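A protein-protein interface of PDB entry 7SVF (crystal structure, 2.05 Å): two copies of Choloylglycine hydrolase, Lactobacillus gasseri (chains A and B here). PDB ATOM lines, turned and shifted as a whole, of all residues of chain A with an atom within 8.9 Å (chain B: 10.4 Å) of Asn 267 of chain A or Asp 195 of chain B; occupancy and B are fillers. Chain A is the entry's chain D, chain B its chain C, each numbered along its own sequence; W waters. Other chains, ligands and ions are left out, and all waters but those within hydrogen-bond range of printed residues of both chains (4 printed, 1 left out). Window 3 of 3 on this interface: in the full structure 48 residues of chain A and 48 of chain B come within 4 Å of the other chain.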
ATOM      1  N   VAL A  22       0.598 -14.292 -19.023  1.00  0.00           N
ATOM      2  CA  VAL A  22       1.460 -15.463 -18.958  1.00  0.00           C
ATOM      3  C   VAL A  22       2.455 -15.434 -20.116  1.00  0.00           C
ATOM      4  O   VAL A  22       2.495 -14.491 -20.910  1.00  0.00           O
ATOM      5  CB  VAL A  22       0.646 -16.771 -18.953  1.00  0.00           C
ATOM      6  CG1 VAL A  22      -0.021 -16.947 -17.589  1.00  0.00           C
ATOM      7  CG2 VAL A  22      -0.388 -16.763 -20.065  1.00  0.00           C
ATOM      8  N   GLY A  23       3.283 -16.475 -20.193  1.00  0.00           N
ATOM      9  CA  GLY A  23       4.352 -16.540 -21.173  1.00  0.00           C
ATOM     10  C   GLY A  23       3.979 -17.265 -22.452  1.00  0.00           C
ATOM     11  O   GLY A  23       4.597 -17.056 -23.504  1.00  0.00           O
ATOM     12  N   GLN A  24       2.954 -18.109 -22.379  1.00  0.00           N
ATOM     13  CA  GLN A  24       2.562 -18.941 -23.505  1.00  0.00           C
ATOM     14  C   GLN A  24       1.079 -19.250 -23.383  1.00  0.00           C
ATOM     15  O   GLN A  24       0.538 -19.321 -22.277  1.00  0.00           O
ATOM     16  CB  GLN A  24       3.372 -20.245 -23.546  1.00  0.00           C
ATOM     17  N   SER A 222       4.749  -2.889 -15.763  1.00  0.00           N
ATOM     18  CA  SER A 222       3.937  -4.059 -15.458  1.00  0.00           C
ATOM     19  C   SER A 222       4.285  -4.717 -14.129  1.00  0.00           C
ATOM     20  O   SER A 222       3.766  -5.807 -13.840  1.00  0.00           O
ATOM     21  CB  SER A 222       4.065  -5.088 -16.587  1.00  0.00           C
ATOM     22  OG  SER A 222       3.402  -4.623 -17.748  1.00  0.00           O
ATOM     23  N   ILE A 223       5.156  -4.108 -13.323  1.00  0.00           N
ATOM     24  CA  ILE A 223       5.425  -4.638 -11.980  1.00  0.00           C
ATOM     25  C   ILE A 223       4.074  -4.778 -11.282  1.00  0.00           C
ATOM     26  O   ILE A 223       3.236  -3.871 -11.384  1.00  0.00           O
ATOM     27  CB  ILE A 223       6.396  -3.731 -11.201  1.00  0.00           C
ATOM     28  CG1 ILE A 223       7.698  -3.546 -11.988  1.00  0.00           C
ATOM     29  CG2 ILE A 223       6.695  -4.297  -9.791  1.00  0.00           C
ATOM     30  CD1 ILE A 223       8.643  -2.532 -11.381  1.00  0.00           C
ATOM     31  N   PRO A 224       3.799  -5.882 -10.578  1.00  0.00           N
ATOM     32  CA  PRO A 224       2.451  -6.051  -9.998  1.00  0.00           C
ATOM     33  C   PRO A 224       2.014  -4.890  -9.110  1.00  0.00           C
ATOM     34  O   PRO A 224       0.859  -4.457  -9.204  1.00  0.00           O
ATOM     35  CB  PRO A 224       2.564  -7.375  -9.207  1.00  0.00           C
ATOM     36  CG  PRO A 224       3.739  -8.091  -9.796  1.00  0.00           C
ATOM     37  CD  PRO A 224       4.697  -7.004 -10.252  1.00  0.00           C
ATOM     38  N   MET A 260      -0.449  -6.160 -20.042  1.00  0.00           N
ATOM     39  CA  MET A 260       0.980  -6.394 -20.209  1.00  0.00           C
ATOM     40  C   MET A 260       1.218  -6.606 -21.704  1.00  0.00           C
ATOM     41  O   MET A 260       0.700  -7.557 -22.292  1.00  0.00           O
ATOM     42  CB  MET A 260       1.403  -7.601 -19.368  1.00  0.00           C
ATOM     43  CG  MET A 260       2.887  -7.843 -19.211  1.00  0.00           C
ATOM     44  SD  MET A 260       3.242  -9.257 -18.109  1.00  0.00           S
ATOM     45  CE  MET A 260       2.391  -8.789 -16.591  1.00  0.00           C
ATOM     46  N   GLY A 263       6.261  -8.120 -25.870  1.00  0.00           N
ATOM     47  CA  GLY A 263       7.539  -7.578 -26.232  1.00  0.00           C
ATOM     48  C   GLY A 263       8.121  -6.608 -25.227  1.00  0.00           C
ATOM     49  O   GLY A 263       9.335  -6.391 -25.239  1.00  0.00           O
ATOM     50  N   SER A 264       7.300  -6.030 -24.347  1.00  0.00           N
ATOM     51  CA  SER A 264       7.798  -5.095 -23.344  1.00  0.00           C
ATOM     52  C   SER A 264       8.244  -5.773 -22.055  1.00  0.00           C
ATOM     53  O   SER A 264       8.814  -5.096 -21.190  1.00  0.00           O
ATOM     54  CB  SER A 264       6.724  -4.048 -23.004  1.00  0.00           C
ATOM     55  OG  SER A 264       5.610  -4.632 -22.326  1.00  0.00           O
ATOM     56  N   VAL A 265       7.986  -7.075 -21.899  1.00  0.00           N
ATOM     57  CA  VAL A 265       8.325  -7.810 -20.682  1.00  0.00           C
ATOM     58  C   VAL A 265       8.920  -9.151 -21.084  1.00  0.00           C
ATOM     59  O   VAL A 265       8.243  -9.970 -21.711  1.00  0.00           O
ATOM     60  CB  VAL A 265       7.107  -8.024 -19.768  1.00  0.00           C
ATOM     61  CG1 VAL A 265       7.488  -8.896 -18.553  1.00  0.00           C
ATOM     62  CG2 VAL A 265       6.527  -6.680 -19.335  1.00  0.00           C
ATOM     63  N   VAL A 266      10.182  -9.375 -20.739  1.00  0.00           N
ATOM     64  CA  VAL A 266      10.859 -10.645 -20.975  1.00  0.00           C
ATOM     65  C   VAL A 266      11.338 -11.164 -19.622  1.00  0.00           C
ATOM     66  O   VAL A 266      12.141 -10.504 -18.953  1.00  0.00           O
ATOM     67  CB  VAL A 266      12.033 -10.498 -21.955  1.00  0.00           C
ATOM     68  CG1 VAL A 266      12.675 -11.842 -22.217  1.00  0.00           C
ATOM     69  CG2 VAL A 266      11.560  -9.860 -23.277  1.00  0.00           C
ATOM     70  N   ASN A 267      10.844 -12.332 -19.212  1.00  0.00           N
ATOM     71  CA  ASN A 267      11.225 -12.846 -17.906  1.00  0.00           C
ATOM     72  C   ASN A 267      12.654 -13.378 -17.949  1.00  0.00           C
ATOM     73  O   ASN A 267      13.308 -13.410 -18.995  1.00  0.00           O
ATOM     74  CB  ASN A 267      10.230 -13.911 -17.419  1.00  0.00           C
ATOM     75  CG  ASN A 267      10.302 -15.238 -18.197  1.00  0.00           C
ATOM     76  OD1 ASN A 267      11.294 -15.583 -18.840  1.00  0.00           O
ATOM     77  ND2 ASN A 267       9.231 -16.002 -18.099  1.00  0.00           N
ATOM     78  N   LYS A 268      13.141 -13.820 -16.788  1.00  0.00           N
ATOM     79  CA  LYS A 268      14.543 -14.193 -16.653  1.00  0.00           C
ATOM     80  C   LYS A 268      14.875 -15.501 -17.354  1.00  0.00           C
ATOM     81  O   LYS A 268      16.060 -15.800 -17.532  1.00  0.00           O
ATOM     82  CB  LYS A 268      14.927 -14.283 -15.172  1.00  0.00           C
ATOM     83  CG  LYS A 268      14.245 -15.437 -14.430  1.00  0.00           C
ATOM     84  CD  LYS A 268      14.818 -15.593 -13.021  1.00  0.00           C
ATOM     85  CE  LYS A 268      14.284 -16.839 -12.332  1.00  0.00           C
ATOM     86  NZ  LYS A 268      12.800 -16.802 -12.207  1.00  0.00           N
ATOM     87  N   LEU A 269      13.872 -16.283 -17.748  1.00  0.00           N
ATOM     88  CA  LEU A 269      14.078 -17.446 -18.593  1.00  0.00           C
ATOM     89  C   LEU A 269      13.947 -17.121 -20.076  1.00  0.00           C
ATOM     90  O   LEU A 269      13.850 -18.043 -20.891  1.00  0.00           O
ATOM     91  CB  LEU A 269      13.095 -18.556 -18.213  1.00  0.00           C
ATOM     92  CG  LEU A 269      13.201 -19.040 -16.764  1.00  0.00           C
ATOM     93  CD1 LEU A 269      12.276 -20.223 -16.527  1.00  0.00           C
ATOM     94  CD2 LEU A 269      14.640 -19.380 -16.411  1.00  0.00           C
ATOM     95  N   GLY A 270      13.934 -15.839 -20.443  1.00  0.00           N
ATOM     96  CA  GLY A 270      13.902 -15.446 -21.839  1.00  0.00           C
ATOM     97  C   GLY A 270      12.543 -15.477 -22.502  1.00  0.00           C
ATOM     98  O   GLY A 270      12.469 -15.355 -23.725  1.00  0.00           O
ATOM     99  N   SER A 271      11.464 -15.616 -21.743  1.00  0.00           N
ATOM    100  CA  SER A 271      10.124 -15.703 -22.298  1.00  0.00           C
ATOM    101  C   SER A 271       9.412 -14.353 -22.225  1.00  0.00           C
ATOM    102  O   SER A 271       9.442 -13.689 -21.182  1.00  0.00           O
ATOM    103  CB  SER A 271       9.325 -16.769 -21.543  1.00  0.00           C
ATOM    104  OG  SER A 271       8.031 -16.902 -22.099  1.00  0.00           O
ATOM    105  N   ASP A 272       8.774 -13.950 -23.333  1.00  0.00           N
ATOM    106  CA  ASP A 272       7.834 -12.831 -23.294  1.00  0.00           C
ATOM    107  C   ASP A 272       6.673 -13.149 -22.358  1.00  0.00           C
ATOM    108  O   ASP A 272       6.143 -14.263 -22.360  1.00  0.00           O
ATOM    109  CB  ASP A 272       7.269 -12.538 -24.690  1.00  0.00           C
ATOM    110  CG  ASP A 272       8.235 -11.783 -25.588  1.00  0.00           C
ATOM    111  OD1 ASP A 272       9.380 -11.511 -25.179  1.00  0.00           O
ATOM    112  OD2 ASP A 272       7.848 -11.473 -26.729  1.00  0.00           O
ATOM    113  N   GLU A 273       6.263 -12.160 -21.564  1.00  0.00           N
ATOM    114  CA  GLU A 273       5.053 -12.250 -20.756  1.00  0.00           C
ATOM    115  C   GLU A 273       4.088 -11.150 -21.169  1.00  0.00           C
ATOM    116  O   GLU A 273       4.494  -9.997 -21.332  1.00  0.00           O
ATOM    117  CB  GLU A 273       5.380 -12.129 -19.273  1.00  0.00           C
ATOM    118  CG  GLU A 273       6.515 -13.021 -18.864  1.00  0.00           C
ATOM    119  CD  GLU A 273       6.023 -14.267 -18.168  1.00  0.00           C
ATOM    120  OE1 GLU A 273       4.790 -14.463 -18.141  1.00  0.00           O
ATOM    121  OE2 GLU A 273       6.866 -15.028 -17.630  1.00  0.00           O
ATOM    122  N   TYR A 274       2.816 -11.497 -21.334  1.00  0.00           N
ATOM    123  CA  TYR A 274       1.878 -10.524 -21.875  1.00  0.00           C
ATOM    124  C   TYR A 274       0.460 -10.991 -21.601  1.00  0.00           C
ATOM    125  O   TYR A 274       0.219 -12.152 -21.256  1.00  0.00           O
ATOM    126  CB  TYR A 274       2.100 -10.313 -23.381  1.00  0.00           C
ATOM    127  CG  TYR A 274       1.912 -11.588 -24.167  1.00  0.00           C
ATOM    128  CD1 TYR A 274       2.947 -12.499 -24.304  1.00  0.00           C
ATOM    129  CD2 TYR A 274       0.680 -11.898 -24.743  1.00  0.00           C
ATOM    130  CE1 TYR A 274       2.778 -13.672 -25.010  1.00  0.00           C
ATOM    131  CE2 TYR A 274       0.497 -13.076 -25.443  1.00  0.00           C
ATOM    132  CZ  TYR A 274       1.553 -13.961 -25.570  1.00  0.00           C
ATOM    133  OH  TYR A 274       1.384 -15.134 -26.268  1.00  0.00           O
ATOM    134  N   GLY B 190      17.535   3.846 -19.751  1.00  0.00           N
ATOM    135  CA  GLY B 190      17.530   2.851 -18.688  1.00  0.00           C
ATOM    136  C   GLY B 190      16.423   1.811 -18.815  1.00  0.00           C
ATOM    137  O   GLY B 190      16.479   0.775 -18.146  1.00  0.00           O
ATOM    138  N   LEU B 191      15.416   2.061 -19.653  1.00  0.00           N
ATOM    139  CA  LEU B 191      14.324   1.101 -19.810  1.00  0.00           C
ATOM    140  C   LEU B 191      14.831  -0.179 -20.463  1.00  0.00           C
ATOM    141  O   LEU B 191      15.599  -0.144 -21.431  1.00  0.00           O
ATOM    142  CB  LEU B 191      13.195   1.697 -20.664  1.00  0.00           C
ATOM    143  CG  LEU B 191      12.346   2.855 -20.115  1.00  0.00           C
ATOM    144  CD1 LEU B 191      11.379   3.344 -21.190  1.00  0.00           C
ATOM    145  CD2 LEU B 191      11.585   2.427 -18.864  1.00  0.00           C
ATOM    146  N   ASP B 192      14.379  -1.320 -19.949  1.00  0.00           N
ATOM    147  CA  ASP B 192      14.812  -2.585 -20.534  1.00  0.00           C
ATOM    148  C   ASP B 192      13.691  -3.607 -20.410  1.00  0.00           C
ATOM    149  O   ASP B 192      13.226  -3.868 -19.294  1.00  0.00           O
ATOM    150  CB  ASP B 192      16.089  -3.067 -19.834  1.00  0.00           C
ATOM    151  CG  ASP B 192      16.663  -4.358 -20.431  1.00  0.00           C
ATOM    152  OD1 ASP B 192      16.075  -4.936 -21.374  1.00  0.00           O
ATOM    153  OD2 ASP B 192      17.717  -4.803 -19.925  1.00  0.00           O
ATOM    154  N   PRO B 193      13.209  -4.178 -21.520  1.00  0.00           N
ATOM    155  CA  PRO B 193      12.168  -5.215 -21.405  1.00  0.00           C
ATOM    156  C   PRO B 193      12.586  -6.403 -20.558  1.00  0.00           C
ATOM    157  O   PRO B 193      11.718  -7.057 -19.967  1.00  0.00           O
ATOM    158  CB  PRO B 193      11.915  -5.622 -22.863  1.00  0.00           C
ATOM    159  CG  PRO B 193      12.301  -4.384 -23.681  1.00  0.00           C
ATOM    160  CD  PRO B 193      13.455  -3.771 -22.923  1.00  0.00           C
ATOM    161  N   HIS B 194      13.881  -6.704 -20.466  1.00  0.00           N
ATOM    162  CA  HIS B 194      14.331  -7.860 -19.695  1.00  0.00           C
ATOM    163  C   HIS B 194      14.200  -7.610 -18.201  1.00  0.00           C
ATOM    164  O   HIS B 194      14.688  -6.600 -17.681  1.00  0.00           O
ATOM    165  CB  HIS B 194      15.783  -8.204 -20.033  1.00  0.00           C
ATOM    166  CG  HIS B 194      15.973  -8.632 -21.452  1.00  0.00           C
ATOM    167  ND1 HIS B 194      15.812  -9.938 -21.863  1.00  0.00           N
ATOM    168  CD2 HIS B 194      16.272  -7.921 -22.564  1.00  0.00           C
ATOM    169  CE1 HIS B 194      16.013 -10.015 -23.168  1.00  0.00           C
ATOM    170  NE2 HIS B 194      16.294  -8.804 -23.617  1.00  0.00           N
ATOM    171  N   ASP B 195      13.571  -8.558 -17.514  1.00  0.00           N
ATOM    172  CA  ASP B 195      13.415  -8.490 -16.071  1.00  0.00           C
ATOM    173  C   ASP B 195      14.769  -8.390 -15.375  1.00  0.00           C
ATOM    174  O   ASP B 195      15.767  -8.971 -15.808  1.00  0.00           O
ATOM    175  CB  ASP B 195      12.692  -9.743 -15.548  1.00  0.00           C
ATOM    176  CG  ASP B 195      11.182  -9.679 -15.700  1.00  0.00           C
ATOM    177  OD1 ASP B 195      10.625  -8.609 -16.017  1.00  0.00           O
ATOM    178  OD2 ASP B 195      10.538 -10.731 -15.493  1.00  0.00           O
ATOM    179  N   ALA B 196      14.787  -7.677 -14.257  1.00  0.00           N
ATOM    180  CA  ALA B 196      15.904  -7.780 -13.338  1.00  0.00           C
ATOM    181  C   ALA B 196      15.848  -9.132 -12.615  1.00  0.00           C
ATOM    182  O   ALA B 196      14.874  -9.885 -12.725  1.00  0.00           O
ATOM    183  CB  ALA B 196      15.882  -6.615 -12.346  1.00  0.00           C
ATOM    184  N   THR B 197      16.918  -9.457 -11.894  1.00  0.00           N
ATOM    185  CA  THR B 197      16.987 -10.705 -11.135  1.00  0.00           C
ATOM    186  C   THR B 197      17.461 -10.395  -9.721  1.00  0.00           C
ATOM    187  O   THR B 197      17.783  -9.248  -9.392  1.00  0.00           O
ATOM    188  CB  THR B 197      17.912 -11.732 -11.806  1.00  0.00           C
ATOM    189  OG1 THR B 197      19.225 -11.174 -11.955  1.00  0.00           O
ATOM    190  CG2 THR B 197      17.368 -12.134 -13.179  1.00  0.00           C
ATOM    191  N   ALA B 198      17.519 -11.439  -8.887  1.00  0.00           N
ATOM    192  CA  ALA B 198      17.773 -11.256  -7.462  1.00  0.00           C
ATOM    193  C   ALA B 198      19.144 -10.638  -7.229  1.00  0.00           C
ATOM    194  O   ALA B 198      20.133 -11.011  -7.870  1.00  0.00           O
ATOM    195  CB  ALA B 198      17.666 -12.593  -6.721  1.00  0.00           C
ATOM    196  N   GLN B 199      19.193  -9.685  -6.300  1.00  0.00           N
ATOM    197  CA  GLN B 199      20.397  -8.957  -5.941  1.00  0.00           C
ATOM    198  C   GLN B 199      20.692  -9.109  -4.449  1.00  0.00           C
ATOM    199  O   GLN B 199      19.821  -9.459  -3.645  1.00  0.00           O
ATOM    200  CB  GLN B 199      20.264  -7.472  -6.289  1.00  0.00           C
ATOM    201  CG  GLN B 199      20.058  -7.240  -7.783  1.00  0.00           C
ATOM    202  CD  GLN B 199      19.372  -5.921  -8.098  1.00  0.00           C
ATOM    203  OE1 GLN B 199      19.249  -5.034  -7.238  1.00  0.00           O
ATOM    204  NE2 GLN B 199      18.928  -5.780  -9.342  1.00  0.00           N
ATOM    205  N   ALA B 207      14.839  -9.066  -4.474  1.00  0.00           N
ATOM    206  CA  ALA B 207      14.487  -9.830  -5.665  1.00  0.00           C
ATOM    207  C   ALA B 207      13.089  -9.455  -6.125  1.00  0.00           C
ATOM    208  O   ALA B 207      12.220  -9.159  -5.295  1.00  0.00           O
ATOM    209  CB  ALA B 207      14.549 -11.343  -5.405  1.00  0.00           C
ATOM    210  N   PRO B 208      12.837  -9.480  -7.437  1.00  0.00           N
ATOM    211  CA  PRO B 208      11.514  -9.098  -7.946  1.00  0.00           C
ATOM    212  C   PRO B 208      10.418  -9.978  -7.369  1.00  0.00           C
ATOM    213  O   PRO B 208      10.622 -11.161  -7.094  1.00  0.00           O
ATOM    214  CB  PRO B 208      11.638  -9.298  -9.466  1.00  0.00           C
ATOM    215  CG  PRO B 208      13.118  -9.320  -9.740  1.00  0.00           C
ATOM    216  CD  PRO B 208      13.738  -9.930  -8.511  1.00  0.00           C
ATOM    217  N   TRP B 209       9.243  -9.385  -7.186  1.00  0.00           N
ATOM    218  CA  TRP B 209       8.058 -10.131  -6.769  1.00  0.00           C
ATOM    219  C   TRP B 209       7.255 -10.636  -7.957  1.00  0.00           C
ATOM    220  O   TRP B 209       6.490 -11.605  -7.826  1.00  0.00           O
ATOM    221  CB  TRP B 209       7.176  -9.240  -5.899  1.00  0.00           C
ATOM    222  CG  TRP B 209       7.844  -8.880  -4.616  1.00  0.00           C
ATOM    223  CD1 TRP B 209       8.329  -7.655  -4.246  1.00  0.00           C
ATOM    224  CD2 TRP B 209       8.114  -9.770  -3.531  1.00  0.00           C
ATOM    225  NE1 TRP B 209       8.875  -7.729  -2.986  1.00  0.00           N
ATOM    226  CE2 TRP B 209       8.759  -9.017  -2.527  1.00  0.00           C
ATOM    227  CE3 TRP B 209       7.867 -11.132  -3.309  1.00  0.00           C
ATOM    228  CZ2 TRP B 209       9.165  -9.580  -1.315  1.00  0.00           C
ATOM    229  CZ3 TRP B 209       8.270 -11.695  -2.097  1.00  0.00           C
ATOM    230  CH2 TRP B 209       8.910 -10.917  -1.119  1.00  0.00           C
ATOM    231  N   GLY B 210       7.426 -10.003  -9.112  1.00  0.00           N
ATOM    232  CA  GLY B 210       6.724 -10.360 -10.324  1.00  0.00           C
ATOM    233  C   GLY B 210       7.536  -9.872 -11.503  1.00  0.00           C
ATOM    234  O   GLY B 210       8.559  -9.206 -11.337  1.00  0.00           O
ATOM    235  N   VAL B 211       7.068 -10.224 -12.708  1.00  0.00           N
ATOM    236  CA  VAL B 211       7.752  -9.796 -13.930  1.00  0.00           C
ATOM    237  C   VAL B 211       7.499  -8.309 -14.182  1.00  0.00           C
ATOM    238  O   VAL B 211       6.516  -7.723 -13.714  1.00  0.00           O
ATOM    239  CB  VAL B 211       7.306 -10.643 -15.139  1.00  0.00           C
ATOM    240  CG1 VAL B 211       7.682 -12.123 -14.959  1.00  0.00           C
ATOM    241  CG2 VAL B 211       5.812 -10.489 -15.380  1.00  0.00           C
ATOM    242  N   GLY B 212       8.393  -7.701 -14.968  1.00  0.00           N
ATOM    243  CA  GLY B 212       8.235  -6.332 -15.426  1.00  0.00           C
ATOM    244  C   GLY B 212       9.225  -5.341 -14.844  1.00  0.00           C
ATOM    245  O   GLY B 212       9.155  -4.147 -15.179  1.00  0.00           O
ATOM    246  N   THR B 213      10.169  -5.797 -14.019  1.00  0.00           N
ATOM    247  CA  THR B 213      11.003  -4.881 -13.243  1.00  0.00           C
ATOM    248  C   THR B 213      11.992  -4.101 -14.098  1.00  0.00           C
ATOM    249  O   THR B 213      12.540  -3.102 -13.624  1.00  0.00           O
ATOM    250  CB  THR B 213      11.772  -5.652 -12.170  1.00  0.00           C
ATOM    251  OG1 THR B 213      12.407  -6.780 -12.779  1.00  0.00           O
ATOM    252  CG2 THR B 213      10.819  -6.138 -11.095  1.00  0.00           C
ATOM    253  N   GLY B 214      12.252  -4.536 -15.333  1.00  0.00           N
ATOM    254  CA  GLY B 214      13.198  -3.811 -16.175  1.00  0.00           C
ATOM    255  C   GLY B 214      12.668  -2.498 -16.711  1.00  0.00           C
ATOM    256  O   GLY B 214      13.457  -1.643 -17.140  1.00  0.00           O
ATOM    257  N   SER B 215      11.347  -2.319 -16.719  1.00  0.00           N
ATOM    258  CA  SER B 215      10.757  -1.078 -17.198  1.00  0.00           C
ATOM    259  C   SER B 215      10.465  -0.098 -16.062  1.00  0.00           C
ATOM    260  O   SER B 215       9.610   0.779 -16.219  1.00  0.00           O
ATOM    261  CB  SER B 215       9.487  -1.379 -17.997  1.00  0.00           C
ATOM    262  OG  SER B 215       9.798  -2.148 -19.146  1.00  0.00           O
ATOM    263  N   LEU B 216      11.129  -0.255 -14.916  1.00  0.00           N
ATOM    264  CA  LEU B 216      11.081   0.742 -13.847  1.00  0.00           C
ATOM    265  C   LEU B 216      11.202   2.163 -14.400  1.00  0.00           C
ATOM    266  O   LEU B 216      12.114   2.465 -15.175  1.00  0.00           O
ATOM    267  CB  LEU B 216      12.213   0.474 -12.849  1.00  0.00           C
ATOM    268  CG  LEU B 216      12.369   1.473 -11.702  1.00  0.00           C
ATOM    269  CD1 LEU B 216      11.154   1.366 -10.780  1.00  0.00           C
ATOM    270  CD2 LEU B 216      13.681   1.222 -10.945  1.00  0.00           C
ATOM    271  N   TYR B 233       8.251   3.137 -26.898  1.00  0.00           N
ATOM    272  CA  TYR B 233       8.823   1.933 -26.313  1.00  0.00           C
ATOM    273  C   TYR B 233       8.024   0.694 -26.701  1.00  0.00           C
ATOM    274  O   TYR B 233       8.598  -0.336 -27.070  1.00  0.00           O
ATOM    275  CB  TYR B 233       8.857   2.108 -24.802  1.00  0.00           C
ATOM    276  CG  TYR B 233       9.517   1.037 -23.968  1.00  0.00           C
ATOM    277  CD1 TYR B 233      10.876   0.772 -24.079  1.00  0.00           C
ATOM    278  CD2 TYR B 233       8.792   0.365 -22.994  1.00  0.00           C
ATOM    279  CE1 TYR B 233      11.490  -0.173 -23.269  1.00  0.00           C
ATOM    280  CE2 TYR B 233       9.400  -0.588 -22.164  1.00  0.00           C
ATOM    281  CZ  TYR B 233      10.740  -0.844 -22.308  1.00  0.00           C
ATOM    282  OH  TYR B 233      11.345  -1.771 -21.491  1.00  0.00           O
HETATM  283  O   HOH W   1       7.019  -3.441 -17.448  1.00  0.00           O
HETATM  284  O   HOH W   2      15.423 -11.786 -19.723  1.00  0.00           O
HETATM  285  O   HOH W   3      11.853 -12.752 -14.293  1.00  0.00           O
HETATM  286  O   HOH W   4       9.203  -4.603 -18.483  1.00  0.00           O
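The backbone carbonyl oxygen (O) of Val 266 of chain A is in hydrogen-bond range of the backbone NH (N) of Asp 195 of chain B, 2.8 Å away.
The backbone carbonyl oxygen of Pro 193 of chain B sits at hydrogen-bond distance from the backbone NH of Val 266 of chain A (2.9 Å).
The backbone carbonyl oxygen of Val 211 of chain B lies close to the backbone carbonyl oxygen of Ser 222 of chain A, 3.4 Å away.
The backbone NH of Ala 196 of chain B is in hydrogen-bond range of the side-chain hydroxyl of Thr 213 of chain B (2.9 Å).
OD1 of Asn 267 of chain A sits at hydrogen-bond distance from N of Leu 269 of chain A (2.9 Å).
The side-chain carboxylate (OD1) of Asp 195 of chain B is in hydrogen-bond range of the backbone NH (N) of Gly 212 of chain B.
OG of Ser 215 of chain B is in hydrogen-bond range of OH of Tyr 233 of chain B.
OD1 of Asn 267 of chain A lies within hydrogen-bond range of N of Ser 271 of chain A (2.9 Å).
The side-chain amide nitrogen of Asn 267 of chain A lies within hydrogen-bond range of the side-chain carboxylate of Glu 273 of chain A (2.6 Å).
Among the printed residues, pairs that only touch across the chains: Asn 267 of chain A with Asp 195 of chain B (3.3 Å), Ser 264 of chain A with Pro 193 of chain B (3.4 Å), Val 266 of chain A with His 194 of chain B (3.5 Å), Val 265 of chain A with Pro 193 of chain B (3.5 Å), Ile 223 of chain A with Gly 212 of chain B (3.6 Å), Gly 263 of chain A with Pro 193 of chain B (3.6 Å), Ile 223 of chain A with Val 211 of chain B (3.7 Å), Ser 264 of chain A with Ser 215 of chain B (3.7 Å), Ile 223 of chain A with Thr 213 of chain B (3.8 Å), Pro 224 of chain A with Gly 210 of chain B (3.8 Å), Lys 268 of chain A with Thr 197 of chain B (3.8 Å), Val 265 of chain A with Val 211 of chain B (3.8 Å), Val 265 of chain A with Gly 212 of chain B (3.9 Å), Met 260 of chain A with Val 211 of chain B (3.9 Å), Asn 267 of chain A with Val 211 of chain B (3.97 Å) and Pro 224 of chain A with Val 211 of chain B (3.98 Å).
Of chain B, only Asp 195 (3.3 Å) and Val 211 (3.97 Å) come within 4 Å of Asn 267 of chain A.
Of chain B, only Pro 193 (2.9 Å), His 194 (3.5 Å) and Asp 195 (2.8 Å) come within 4 Å of Val 266 of chain A.
No residue of chain B comes within 4 Å of Leu 269 of chain A.
No residue of chain B comes within 4 Å of Ser 271 of chain A.
No residue of chain A comes within 4 Å of Ala 196 of chain B.
Val 211 of chain B touches just these residues of chain A: Ser 222, Ile 223, Pro 224, Met 260, Val 265 and Asn 267.
Of the printed residues of chain B, Gly 263 of chain A touches Pro 193 (3.6 Å).
Of the printed residues of chain B, Ser 222 of chain A touches Val 211.
Printed residues of chain A within 4 Å of His 194 of chain B: Val 266 (3.5 Å).
Printed residues of chain A within 4 Å of Pro 193 of chain B: Gly 263 (3.6 Å), Ser 264 (3.4 Å), Val 265 (3.5 Å) and Val 266 (2.9 Å).
The nearest residue of chain B that does not touch Asn 267 of chain A is His 194 of chain B (5.2 Å).
Hydrophobic or aromatic side chains of chain B within 4 Å of the printed part of chain A: Pro 193, His 194 and Val 211.
Printed residues of chain A that touch a printed residue of chain B: Ser 222, Ile 223, Pro 224, Met 260, Gly 263, Ser 264, Val 265, Val 266, Asn 267 and Lys 268.
Hydrophobic or aromatic side chains of chain A within 4 Å of the printed part of chain B: Ile 223, Pro 224, Met 260, Val 265 and Val 266.
Among the printed residues, no Asp or Glu carboxylate lies within 4 Å of a Lys or Arg side-chain nitrogen of the other chain.
No position is printed for both chains.
Of the 19 pairs that touch across the chains among the printed residues, none has its exchanged pair printed and touching as well.
Water W4 lies within hydrogen-bond range of OG of Ser 215 of chain B, O of Ser 264 of chain A and O of Gly 212 of chain B.
Water W3 lies within hydrogen-bond range of the side-chain carboxylate (OD2) of Asp 195 of chain B (2.7 Å) and the backbone NH (N) of Lys 268 of chain A (3.0 Å).
Water W2 bridges O of Asn 267 of chain A (2.8 Å) and ND1 of His 194 of chain B (2.9 Å).
Water W1 lies within hydrogen-bond range of the backbone NH of Ser 222 of chain A and the backbone carbonyl oxygen of Gly 212 of chain B.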
